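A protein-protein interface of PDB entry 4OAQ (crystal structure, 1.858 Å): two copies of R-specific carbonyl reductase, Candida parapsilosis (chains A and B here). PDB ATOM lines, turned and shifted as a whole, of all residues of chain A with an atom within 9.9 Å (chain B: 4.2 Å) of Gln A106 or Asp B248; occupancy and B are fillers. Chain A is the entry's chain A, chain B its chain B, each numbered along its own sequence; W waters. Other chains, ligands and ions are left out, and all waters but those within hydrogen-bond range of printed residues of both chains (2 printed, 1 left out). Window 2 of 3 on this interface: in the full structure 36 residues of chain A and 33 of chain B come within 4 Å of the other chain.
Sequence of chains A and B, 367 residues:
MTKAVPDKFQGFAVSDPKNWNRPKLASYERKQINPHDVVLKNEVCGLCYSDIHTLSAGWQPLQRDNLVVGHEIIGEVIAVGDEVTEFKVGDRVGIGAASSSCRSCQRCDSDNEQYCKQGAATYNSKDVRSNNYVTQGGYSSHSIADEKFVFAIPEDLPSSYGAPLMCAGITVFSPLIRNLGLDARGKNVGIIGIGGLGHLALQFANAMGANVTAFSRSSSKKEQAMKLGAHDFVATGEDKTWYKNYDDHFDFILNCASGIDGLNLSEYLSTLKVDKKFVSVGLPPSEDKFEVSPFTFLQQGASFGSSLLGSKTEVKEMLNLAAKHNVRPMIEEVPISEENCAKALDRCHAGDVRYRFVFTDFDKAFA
No position is printed for both chains.
Of the 5 pairs that touch across the chains among the printed residues, none has its exchanged pair printed and touching as well.
Water W1 lies within hydrogen-bond range of the side-chain carboxylate of Asp B248 (2.7 Å), the backbone NH of Gln A106 (3.2 Å) and the backbone NH of Arg A107 (3.3 Å).
Water W2 lies within hydrogen-bond range of the backbone NH (N) of Asp B248 (2.7 Å), the backbone carbonyl oxygen (O) of Leu B272 (2.8 Å) and the guanidinium group (NH2) of Arg A107 (3.3 Å).
Gln A106 touches one residue of chain B.
Of the printed residues of chain B, Arg A107 touches Asp B248 (3.0 Å), Leu B272 (2.9 Å) and Lys B273 (3.9 Å).
Of the printed residues of chain B, Lys A117 touches Asp B247.
Of chain A, only Lys A117 comes within 4 Å of Asp B247.
Of the printed residues of chain A, Asp B248 touches Gln A106 and Arg A107.
Of the printed residues of chain A, Leu B272 touches Arg A107 (2.9 Å).
Lys B273 touches just one residue of chain A: Arg A107 (3.9 Å).
The nearest printed residue of chain B that does not touch Gln A106 is Lys B273 (6.5 Å).
The nearest residue of chain A that does not touch Asp B248 is Cys A105 (6.2 Å).
The side-chain sulfur of Cys A105 lies close to the backbone NH of Arg A107 (3.7 Å).
The backbone NH of Asn A112 is in hydrogen-bond range of the backbone carbonyl oxygen of Arg A107 (2.9 Å).
The backbone carbonyl oxygen (O) of Arg A107 is in hydrogen-bond range of the backbone NH (N) of Glu A113 (3.3 Å).
The guanidinium group of Arg A107 is in hydrogen-bond range of the backbone carbonyl oxygen of Tyr A115, at 3.1 Å.
The backbone carbonyl oxygen of Asp B248 lies within hydrogen-bond range of the side-chain amino group of Lys B273 (2.8 Å).
The backbone carbonyl oxygen of Phe B250 sits at hydrogen-bond distance from the backbone NH of Lys B273 (2.8 Å).
Of the 18 printed residues of chain A, 3 touch a printed residue of chain B.
Of the 8 printed residues of chain B, 4 touch a printed residue of chain A.
Printed residues of chain B that touch a printed residue of chain A: Asp B247, Asp B248, Leu B272 and Lys B273.
Along chain B the printed residues that touch a printed residue of chain A span positions 247 to 273.
Among the printed residues, 5 pairs touch across the chains.
Among the printed residues, Asp or Glu carboxylates within 4 Å of a Lys or Arg side-chain nitrogen of the other chain: Arg A107 with Asp B248.
The side-chain carboxylate (OD1) of Asp B248 is in salt-bridge range of the guanidinium group (NE) of Arg A107, 3.0 Å away.
The guanidinium group (NH2) of Arg A107 lies within hydrogen-bond range of the backbone carbonyl oxygen (O) of Leu B272 (2.9 Å).
Among the printed residues, merely in contact across the chains: Gln A106 with Asp B248, Arg A107 with Lys B273 and Lys A117 with Asp B247.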
ATOM      1  N   SER A 101      20.946   2.785 -26.090  1.00  0.00           N
ATOM      2  CA  SER A 101      21.883   1.689 -26.311  1.00  0.00           C
ATOM      3  C   SER A 101      23.281   2.260 -26.557  1.00  0.00           C
ATOM      4  O   SER A 101      23.461   3.474 -26.567  1.00  0.00           O
ATOM      5  CB  SER A 101      21.421   0.814 -27.472  1.00  0.00           C
ATOM      6  OG  SER A 101      21.427   1.517 -28.704  1.00  0.00           O
ATOM      7  N   CYS A 102      24.278   1.410 -26.752  1.00  0.00           N
ATOM      8  CA  CYS A 102      25.651   1.919 -26.822  1.00  0.00           C
ATOM      9  C   CYS A 102      26.053   2.582 -28.154  1.00  0.00           C
ATOM     10  O   CYS A 102      27.017   3.350 -28.202  1.00  0.00           O
ATOM     11  CB  CYS A 102      26.647   0.815 -26.455  1.00  0.00           C
ATOM     12  SG  CYS A 102      27.015  -0.403 -27.762  1.00  0.00           S
ATOM     13  N   ARG A 103      25.322   2.284 -29.225  1.00  0.00           N
ATOM     14  CA  ARG A 103      25.676   2.774 -30.566  1.00  0.00           C
ATOM     15  C   ARG A 103      27.043   2.300 -31.061  1.00  0.00           C
ATOM     16  O   ARG A 103      27.616   2.892 -31.985  1.00  0.00           O
ATOM     17  CB  ARG A 103      25.603   4.309 -30.619  1.00  0.00           C
ATOM     18  CG  ARG A 103      24.172   4.837 -30.609  1.00  0.00           C
ATOM     19  CD  ARG A 103      24.136   6.351 -30.707  1.00  0.00           C
ATOM     20  NE  ARG A 103      22.750   6.785 -30.819  1.00  0.00           N
ATOM     21  CZ  ARG A 103      22.129   6.935 -31.979  1.00  0.00           C
ATOM     22  NH1 ARG A 103      22.797   6.720 -33.102  1.00  0.00           N
ATOM     23  NH2 ARG A 103      20.855   7.306 -32.012  1.00  0.00           N
ATOM     24  N   SER A 104      27.574   1.241 -30.456  1.00  0.00           N
ATOM     25  CA  SER A 104      28.918   0.788 -30.814  1.00  0.00           C
ATOM     26  C   SER A 104      29.103  -0.709 -30.642  1.00  0.00           C
ATOM     27  O   SER A 104      30.185  -1.173 -30.289  1.00  0.00           O
ATOM     28  CB  SER A 104      29.980   1.538 -30.005  1.00  0.00           C
ATOM     29  OG  SER A 104      30.227   0.876 -28.780  1.00  0.00           O
ATOM     30  N   CYS A 105      28.049  -1.465 -30.912  1.00  0.00           N
ATOM     31  CA  CYS A 105      28.159  -2.913 -30.911  1.00  0.00           C
ATOM     32  C   CYS A 105      27.422  -3.443 -32.124  1.00  0.00           C
ATOM     33  O   CYS A 105      26.748  -2.691 -32.825  1.00  0.00           O
ATOM     34  CB  CYS A 105      27.574  -3.494 -29.626  1.00  0.00           C
ATOM     35  SG  CYS A 105      25.770  -3.462 -29.546  1.00  0.00           S
ATOM     36  N   GLN A 106      27.533  -4.740 -32.375  1.00  0.00           N
ATOM     37  CA  GLN A 106      26.918  -5.302 -33.565  1.00  0.00           C
ATOM     38  C   GLN A 106      25.397  -5.318 -33.479  1.00  0.00           C
ATOM     39  O   GLN A 106      24.736  -5.024 -34.469  1.00  0.00           O
ATOM     40  CB  GLN A 106      27.451  -6.703 -33.866  1.00  0.00           C
ATOM     41  CG  GLN A 106      26.980  -7.267 -35.201  1.00  0.00           C
ATOM     42  CD  GLN A 106      27.429  -6.433 -36.400  1.00  0.00           C
ATOM     43  OE1 GLN A 106      28.594  -6.038 -36.497  1.00  0.00           O
ATOM     44  NE2 GLN A 106      26.502  -6.174 -37.323  1.00  0.00           N
ATOM     45  N   ARG A 107      24.860  -5.668 -32.312  1.00  0.00           N
ATOM     46  CA  ARG A 107      23.415  -5.607 -32.060  1.00  0.00           C
ATOM     47  C   ARG A 107      22.810  -4.253 -32.368  1.00  0.00           C
ATOM     48  O   ARG A 107      21.732  -4.162 -32.959  1.00  0.00           O
ATOM     49  CB  ARG A 107      23.106  -6.002 -30.606  1.00  0.00           C
ATOM     50  CG  ARG A 107      23.471  -7.441 -30.335  1.00  0.00           C
ATOM     51  CD  ARG A 107      23.341  -7.831 -28.886  1.00  0.00           C
ATOM     52  NE  ARG A 107      23.746  -9.222 -28.714  1.00  0.00           N
ATOM     53  CZ  ARG A 107      23.384 -10.006 -27.700  1.00  0.00           C
ATOM     54  NH1 ARG A 107      22.583  -9.548 -26.738  1.00  0.00           N
ATOM     55  NH2 ARG A 107      23.800 -11.259 -27.671  1.00  0.00           N
ATOM     56  N   CYS A 108      23.498  -3.200 -31.961  1.00  0.00           N
ATOM     57  CA  CYS A 108      23.025  -1.853 -32.216  1.00  0.00           C
ATOM     58  C   CYS A 108      22.950  -1.550 -33.709  1.00  0.00           C
ATOM     59  O   CYS A 108      22.124  -0.752 -34.131  1.00  0.00           O
ATOM     60  CB  CYS A 108      23.924  -0.834 -31.511  1.00  0.00           C
ATOM     61  SG  CYS A 108      23.502  -0.604 -29.762  1.00  0.00           S
ATOM     62  N   ASP A 109      23.793  -2.191 -34.511  1.00  0.00           N
ATOM     63  CA  ASP A 109      23.796  -1.916 -35.950  1.00  0.00           C
ATOM     64  C   ASP A 109      23.095  -2.989 -36.789  1.00  0.00           C
ATOM     65  O   ASP A 109      23.208  -2.996 -38.012  1.00  0.00           O
ATOM     66  CB  ASP A 109      25.224  -1.698 -36.468  1.00  0.00           C
ATOM     67  N   SER A 110      22.373  -3.894 -36.144  1.00  0.00           N
ATOM     68  CA  SER A 110      21.712  -4.955 -36.895  1.00  0.00           C
ATOM     69  C   SER A 110      20.323  -5.254 -36.347  1.00  0.00           C
ATOM     70  O   SER A 110      19.917  -6.413 -36.241  1.00  0.00           O
ATOM     71  CB  SER A 110      22.590  -6.215 -36.935  1.00  0.00           C
ATOM     72  OG  SER A 110      23.270  -6.394 -35.708  1.00  0.00           O
ATOM     73  N   ASP A 111      19.599  -4.195 -35.995  1.00  0.00           N
ATOM     74  CA  ASP A 111      18.204  -4.309 -35.565  1.00  0.00           C
ATOM     75  C   ASP A 111      18.061  -5.211 -34.341  1.00  0.00           C
ATOM     76  O   ASP A 111      17.107  -5.973 -34.226  1.00  0.00           O
ATOM     77  CB  ASP A 111      17.318  -4.831 -36.710  1.00  0.00           C
ATOM     78  CG  ASP A 111      17.312  -3.912 -37.918  1.00  0.00           C
ATOM     79  OD1 ASP A 111      17.307  -2.678 -37.723  1.00  0.00           O
ATOM     80  OD2 ASP A 111      17.310  -4.436 -39.061  1.00  0.00           O
ATOM     81  N   ASN A 112      19.035  -5.156 -33.445  1.00  0.00           N
ATOM     82  CA  ASN A 112      18.892  -5.829 -32.156  1.00  0.00           C
ATOM     83  C   ASN A 112      19.259  -4.879 -31.030  1.00  0.00           C
ATOM     84  O   ASN A 112      19.735  -5.297 -29.971  1.00  0.00           O
ATOM     85  CB  ASN A 112      19.717  -7.118 -32.105  1.00  0.00           C
ATOM     86  CG  ASN A 112      18.934  -8.316 -32.588  1.00  0.00           C
ATOM     87  OD1 ASN A 112      17.736  -8.420 -32.334  1.00  0.00           O
ATOM     88  ND2 ASN A 112      19.600  -9.223 -33.291  1.00  0.00           N
ATOM     89  N   GLU A 113      19.004  -3.593 -31.250  1.00  0.00           N
ATOM     90  CA  GLU A 113      19.439  -2.574 -30.308  1.00  0.00           C
ATOM     91  C   GLU A 113      18.753  -2.738 -28.943  1.00  0.00           C
ATOM     92  O   GLU A 113      19.249  -2.238 -27.932  1.00  0.00           O
ATOM     93  CB  GLU A 113      19.221  -1.167 -30.891  1.00  0.00           C
ATOM     94  CG  GLU A 113      17.743  -0.792 -31.138  1.00  0.00           C
ATOM     95  CD  GLU A 113      17.218  -1.239 -32.504  1.00  0.00           C
ATOM     96  OE1 GLU A 113      17.941  -1.952 -33.227  1.00  0.00           O
ATOM     97  OE2 GLU A 113      16.082  -0.852 -32.876  1.00  0.00           O
ATOM     98  N   GLN A 114      17.624  -3.447 -28.908  1.00  0.00           N
ATOM     99  CA  GLN A 114      16.908  -3.648 -27.648  1.00  0.00           C
ATOM    100  C   GLN A 114      17.688  -4.674 -26.828  1.00  0.00           C
ATOM    101  O   GLN A 114      17.556  -4.740 -25.621  1.00  0.00           O
ATOM    102  CB  GLN A 114      15.444  -4.100 -27.888  1.00  0.00           C
ATOM    103  CG  GLN A 114      15.266  -5.560 -28.438  1.00  0.00           C
ATOM    104  CD  GLN A 114      15.399  -5.668 -29.959  1.00  0.00           C
ATOM    105  OE1 GLN A 114      15.985  -4.792 -30.615  1.00  0.00           O
ATOM    106  NE2 GLN A 114      14.857  -6.751 -30.528  1.00  0.00           N
ATOM    107  N   TYR A 115      18.537  -5.450 -27.494  1.00  0.00           N
ATOM    108  CA  TYR A 115      19.427  -6.386 -26.806  1.00  0.00           C
ATOM    109  C   TYR A 115      20.827  -5.853 -26.530  1.00  0.00           C
ATOM    110  O   TYR A 115      21.727  -6.623 -26.188  1.00  0.00           O
ATOM    111  CB  TYR A 115      19.543  -7.687 -27.593  1.00  0.00           C
ATOM    112  CG  TYR A 115      18.259  -8.503 -27.582  1.00  0.00           C
ATOM    113  CD1 TYR A 115      17.868  -9.190 -26.442  1.00  0.00           C
ATOM    114  CD2 TYR A 115      17.459  -8.598 -28.714  1.00  0.00           C
ATOM    115  CE1 TYR A 115      16.692  -9.948 -26.425  1.00  0.00           C
ATOM    116  CE2 TYR A 115      16.287  -9.351 -28.705  1.00  0.00           C
ATOM    117  CZ  TYR A 115      15.913 -10.012 -27.562  1.00  0.00           C
ATOM    118  OH  TYR A 115      14.760 -10.745 -27.543  1.00  0.00           O
ATOM    119  N   CYS A 116      21.041  -4.551 -26.682  1.00  0.00           N
ATOM    120  CA  CYS A 116      22.372  -4.016 -26.376  1.00  0.00           C
ATOM    121  C   CYS A 116      22.762  -4.361 -24.943  1.00  0.00           C
ATOM    122  O   CYS A 116      21.962  -4.205 -24.030  1.00  0.00           O
ATOM    123  CB  CYS A 116      22.429  -2.508 -26.561  1.00  0.00           C
ATOM    124  SG  CYS A 116      24.068  -1.864 -26.304  1.00  0.00           S
ATOM    125  N   LYS A 117      23.984  -4.848 -24.759  1.00  0.00           N
ATOM    126  CA  LYS A 117      24.456  -5.245 -23.439  1.00  0.00           C
ATOM    127  C   LYS A 117      24.483  -4.046 -22.490  1.00  0.00           C
ATOM    128  O   LYS A 117      24.361  -4.196 -21.273  1.00  0.00           O
ATOM    129  CB  LYS A 117      25.845  -5.837 -23.566  1.00  0.00           C
ATOM    130  CG  LYS A 117      26.423  -6.334 -22.268  1.00  0.00           C
ATOM    131  CD  LYS A 117      27.792  -6.909 -22.526  1.00  0.00           C
ATOM    132  N   LYS A 148      17.146   6.274 -31.553  1.00  0.00           N
ATOM    133  CA  LYS A 148      16.974   4.876 -31.946  1.00  0.00           C
ATOM    134  C   LYS A 148      15.800   4.220 -31.213  1.00  0.00           C
ATOM    135  O   LYS A 148      15.343   3.147 -31.602  1.00  0.00           O
ATOM    136  CB  LYS A 148      18.262   4.074 -31.679  1.00  0.00           C
ATOM    137  CG  LYS A 148      19.356   4.223 -32.760  1.00  0.00           C
ATOM    138  CD  LYS A 148      20.642   3.500 -32.349  1.00  0.00           C
ATOM    139  CE  LYS A 148      20.969   2.306 -33.257  1.00  0.00           C
ATOM    140  NZ  LYS A 148      21.296   2.710 -34.662  1.00  0.00           N
ATOM    141  N   TYR B 246      33.854 -13.553 -24.757  1.00  0.00           N
ATOM    142  CA  TYR B 246      32.955 -14.184 -25.732  1.00  0.00           C
ATOM    143  C   TYR B 246      31.605 -13.500 -25.813  1.00  0.00           C
ATOM    144  O   TYR B 246      30.596 -14.142 -26.084  1.00  0.00           O
ATOM    145  CB  TYR B 246      32.753 -15.669 -25.410  1.00  0.00           C
ATOM    146  CG  TYR B 246      34.004 -16.478 -25.602  1.00  0.00           C
ATOM    147  CD1 TYR B 246      34.180 -17.257 -26.733  1.00  0.00           C
ATOM    148  CD2 TYR B 246      35.014 -16.453 -24.660  1.00  0.00           C
ATOM    149  CE1 TYR B 246      35.328 -17.990 -26.918  1.00  0.00           C
ATOM    150  CE2 TYR B 246      36.171 -17.181 -24.836  1.00  0.00           C
ATOM    151  CZ  TYR B 246      36.324 -17.947 -25.966  1.00  0.00           C
ATOM    152  OH  TYR B 246      37.477 -18.677 -26.146  1.00  0.00           O
ATOM    153  N   ASP B 247      31.571 -12.192 -25.603  1.00  0.00           N
ATOM    154  CA  ASP B 247      30.330 -11.470 -25.827  1.00  0.00           C
ATOM    155  C   ASP B 247      29.814 -11.658 -27.256  1.00  0.00           C
ATOM    156  O   ASP B 247      30.582 -11.516 -28.209  1.00  0.00           O
ATOM    157  CB  ASP B 247      30.514  -9.971 -25.589  1.00  0.00           C
ATOM    158  CG  ASP B 247      29.211  -9.220 -25.698  1.00  0.00           C
ATOM    159  OD1 ASP B 247      28.258  -9.593 -24.975  1.00  0.00           O
ATOM    160  OD2 ASP B 247      29.111  -8.279 -26.515  1.00  0.00           O
ATOM    161  N   ASP B 248      28.528 -12.004 -27.383  1.00  0.00           N
ATOM    162  CA  ASP B 248      27.814 -12.002 -28.667  1.00  0.00           C
ATOM    163  C   ASP B 248      28.500 -12.909 -29.677  1.00  0.00           C
ATOM    164  O   ASP B 248      28.595 -12.588 -30.862  1.00  0.00           O
ATOM    165  CB  ASP B 248      27.700 -10.568 -29.200  1.00  0.00           C
ATOM    166  CG  ASP B 248      26.651 -10.411 -30.293  1.00  0.00           C
ATOM    167  OD1 ASP B 248      25.585 -11.079 -30.255  1.00  0.00           O
ATOM    168  OD2 ASP B 248      26.892  -9.578 -31.199  1.00  0.00           O
ATOM    169  N   HIS B 249      28.926 -14.076 -29.213  1.00  0.00           N
ATOM    170  CA  HIS B 249      29.830 -14.893 -30.009  1.00  0.00           C
ATOM    171  C   HIS B 249      29.235 -16.138 -30.655  1.00  0.00           C
ATOM    172  O   HIS B 249      29.489 -16.406 -31.837  1.00  0.00           O
ATOM    173  CB  HIS B 249      31.002 -15.308 -29.148  1.00  0.00           C
ATOM    174  CG  HIS B 249      32.004 -16.144 -29.869  1.00  0.00           C
ATOM    175  ND1 HIS B 249      33.009 -15.601 -30.641  1.00  0.00           N
ATOM    176  CD2 HIS B 249      32.151 -17.493 -29.944  1.00  0.00           C
ATOM    177  CE1 HIS B 249      33.748 -16.580 -31.146  1.00  0.00           C
ATOM    178  NE2 HIS B 249      33.247 -17.733 -30.737  1.00  0.00           N
ATOM    179  N   PHE B 250      28.472 -16.903 -29.877  1.00  0.00           N
ATOM    180  CA  PHE B 250      28.047 -18.233 -30.296  1.00  0.00           C
ATOM    181  C   PHE B 250      26.716 -18.268 -31.015  1.00  0.00           C
ATOM    182  O   PHE B 250      25.722 -17.661 -30.574  1.00  0.00           O
ATOM    183  CB  PHE B 250      27.962 -19.168 -29.090  1.00  0.00           C
ATOM    184  CG  PHE B 250      29.299 -19.500 -28.492  1.00  0.00           C
ATOM    185  CD1 PHE B 250      30.143 -20.398 -29.111  1.00  0.00           C
ATOM    186  CD2 PHE B 250      29.712 -18.914 -27.314  1.00  0.00           C
ATOM    187  CE1 PHE B 250      31.388 -20.715 -28.550  1.00  0.00           C
ATOM    188  CE2 PHE B 250      30.951 -19.219 -26.761  1.00  0.00           C
ATOM    189  CZ  PHE B 250      31.787 -20.119 -27.383  1.00  0.00           C
ATOM    190  N   THR B 271      26.913 -15.537 -23.586  1.00  0.00           N
ATOM    191  CA  THR B 271      27.854 -15.497 -24.714  1.00  0.00           C
ATOM    192  C   THR B 271      27.189 -15.847 -26.041  1.00  0.00           C
ATOM    193  O   THR B 271      27.877 -15.947 -27.063  1.00  0.00           O
ATOM    194  CB  THR B 271      29.022 -16.489 -24.525  1.00  0.00           C
ATOM    195  OG1 THR B 271      28.523 -17.837 -24.580  1.00  0.00           O
ATOM    196  CG2 THR B 271      29.742 -16.248 -23.197  1.00  0.00           C
ATOM    197  N   LEU B 272      25.871 -16.053 -26.030  1.00  0.00           N
ATOM    198  CA  LEU B 272      25.151 -16.354 -27.268  1.00  0.00           C
ATOM    199  C   LEU B 272      24.869 -15.110 -28.093  1.00  0.00           C
ATOM    200  O   LEU B 272      24.730 -14.009 -27.559  1.00  0.00           O
ATOM    201  CB  LEU B 272      23.815 -17.047 -26.976  1.00  0.00           C
ATOM    202  CG  LEU B 272      23.875 -18.497 -26.478  1.00  0.00           C
ATOM    203  CD1 LEU B 272      22.522 -18.907 -25.930  1.00  0.00           C
ATOM    204  CD2 LEU B 272      24.331 -19.460 -27.595  1.00  0.00           C
ATOM    205  N   LYS B 273      24.744 -15.282 -29.403  1.00  0.00           N
ATOM    206  CA  LYS B 273      24.156 -14.224 -30.197  1.00  0.00           C
ATOM    207  C   LYS B 273      22.668 -14.219 -29.887  1.00  0.00           C
ATOM    208  O   LYS B 273      22.165 -15.113 -29.186  1.00  0.00           O
ATOM    209  CB  LYS B 273      24.376 -14.493 -31.682  1.00  0.00           C
ATOM    210  CG  LYS B 273      25.844 -14.432 -32.096  1.00  0.00           C
ATOM    211  CD  LYS B 273      26.034 -14.745 -33.575  1.00  0.00           C
ATOM    212  CE  LYS B 273      27.502 -14.689 -33.952  1.00  0.00           C
ATOM    213  NZ  LYS B 273      28.120 -13.415 -33.539  1.00  0.00           N
HETATM  214  O   HOH W   1      26.972  -7.073 -30.251  1.00  0.00           O
HETATM  215  O   HOH W   2      26.321 -12.405 -25.893  1.00  0.00           O
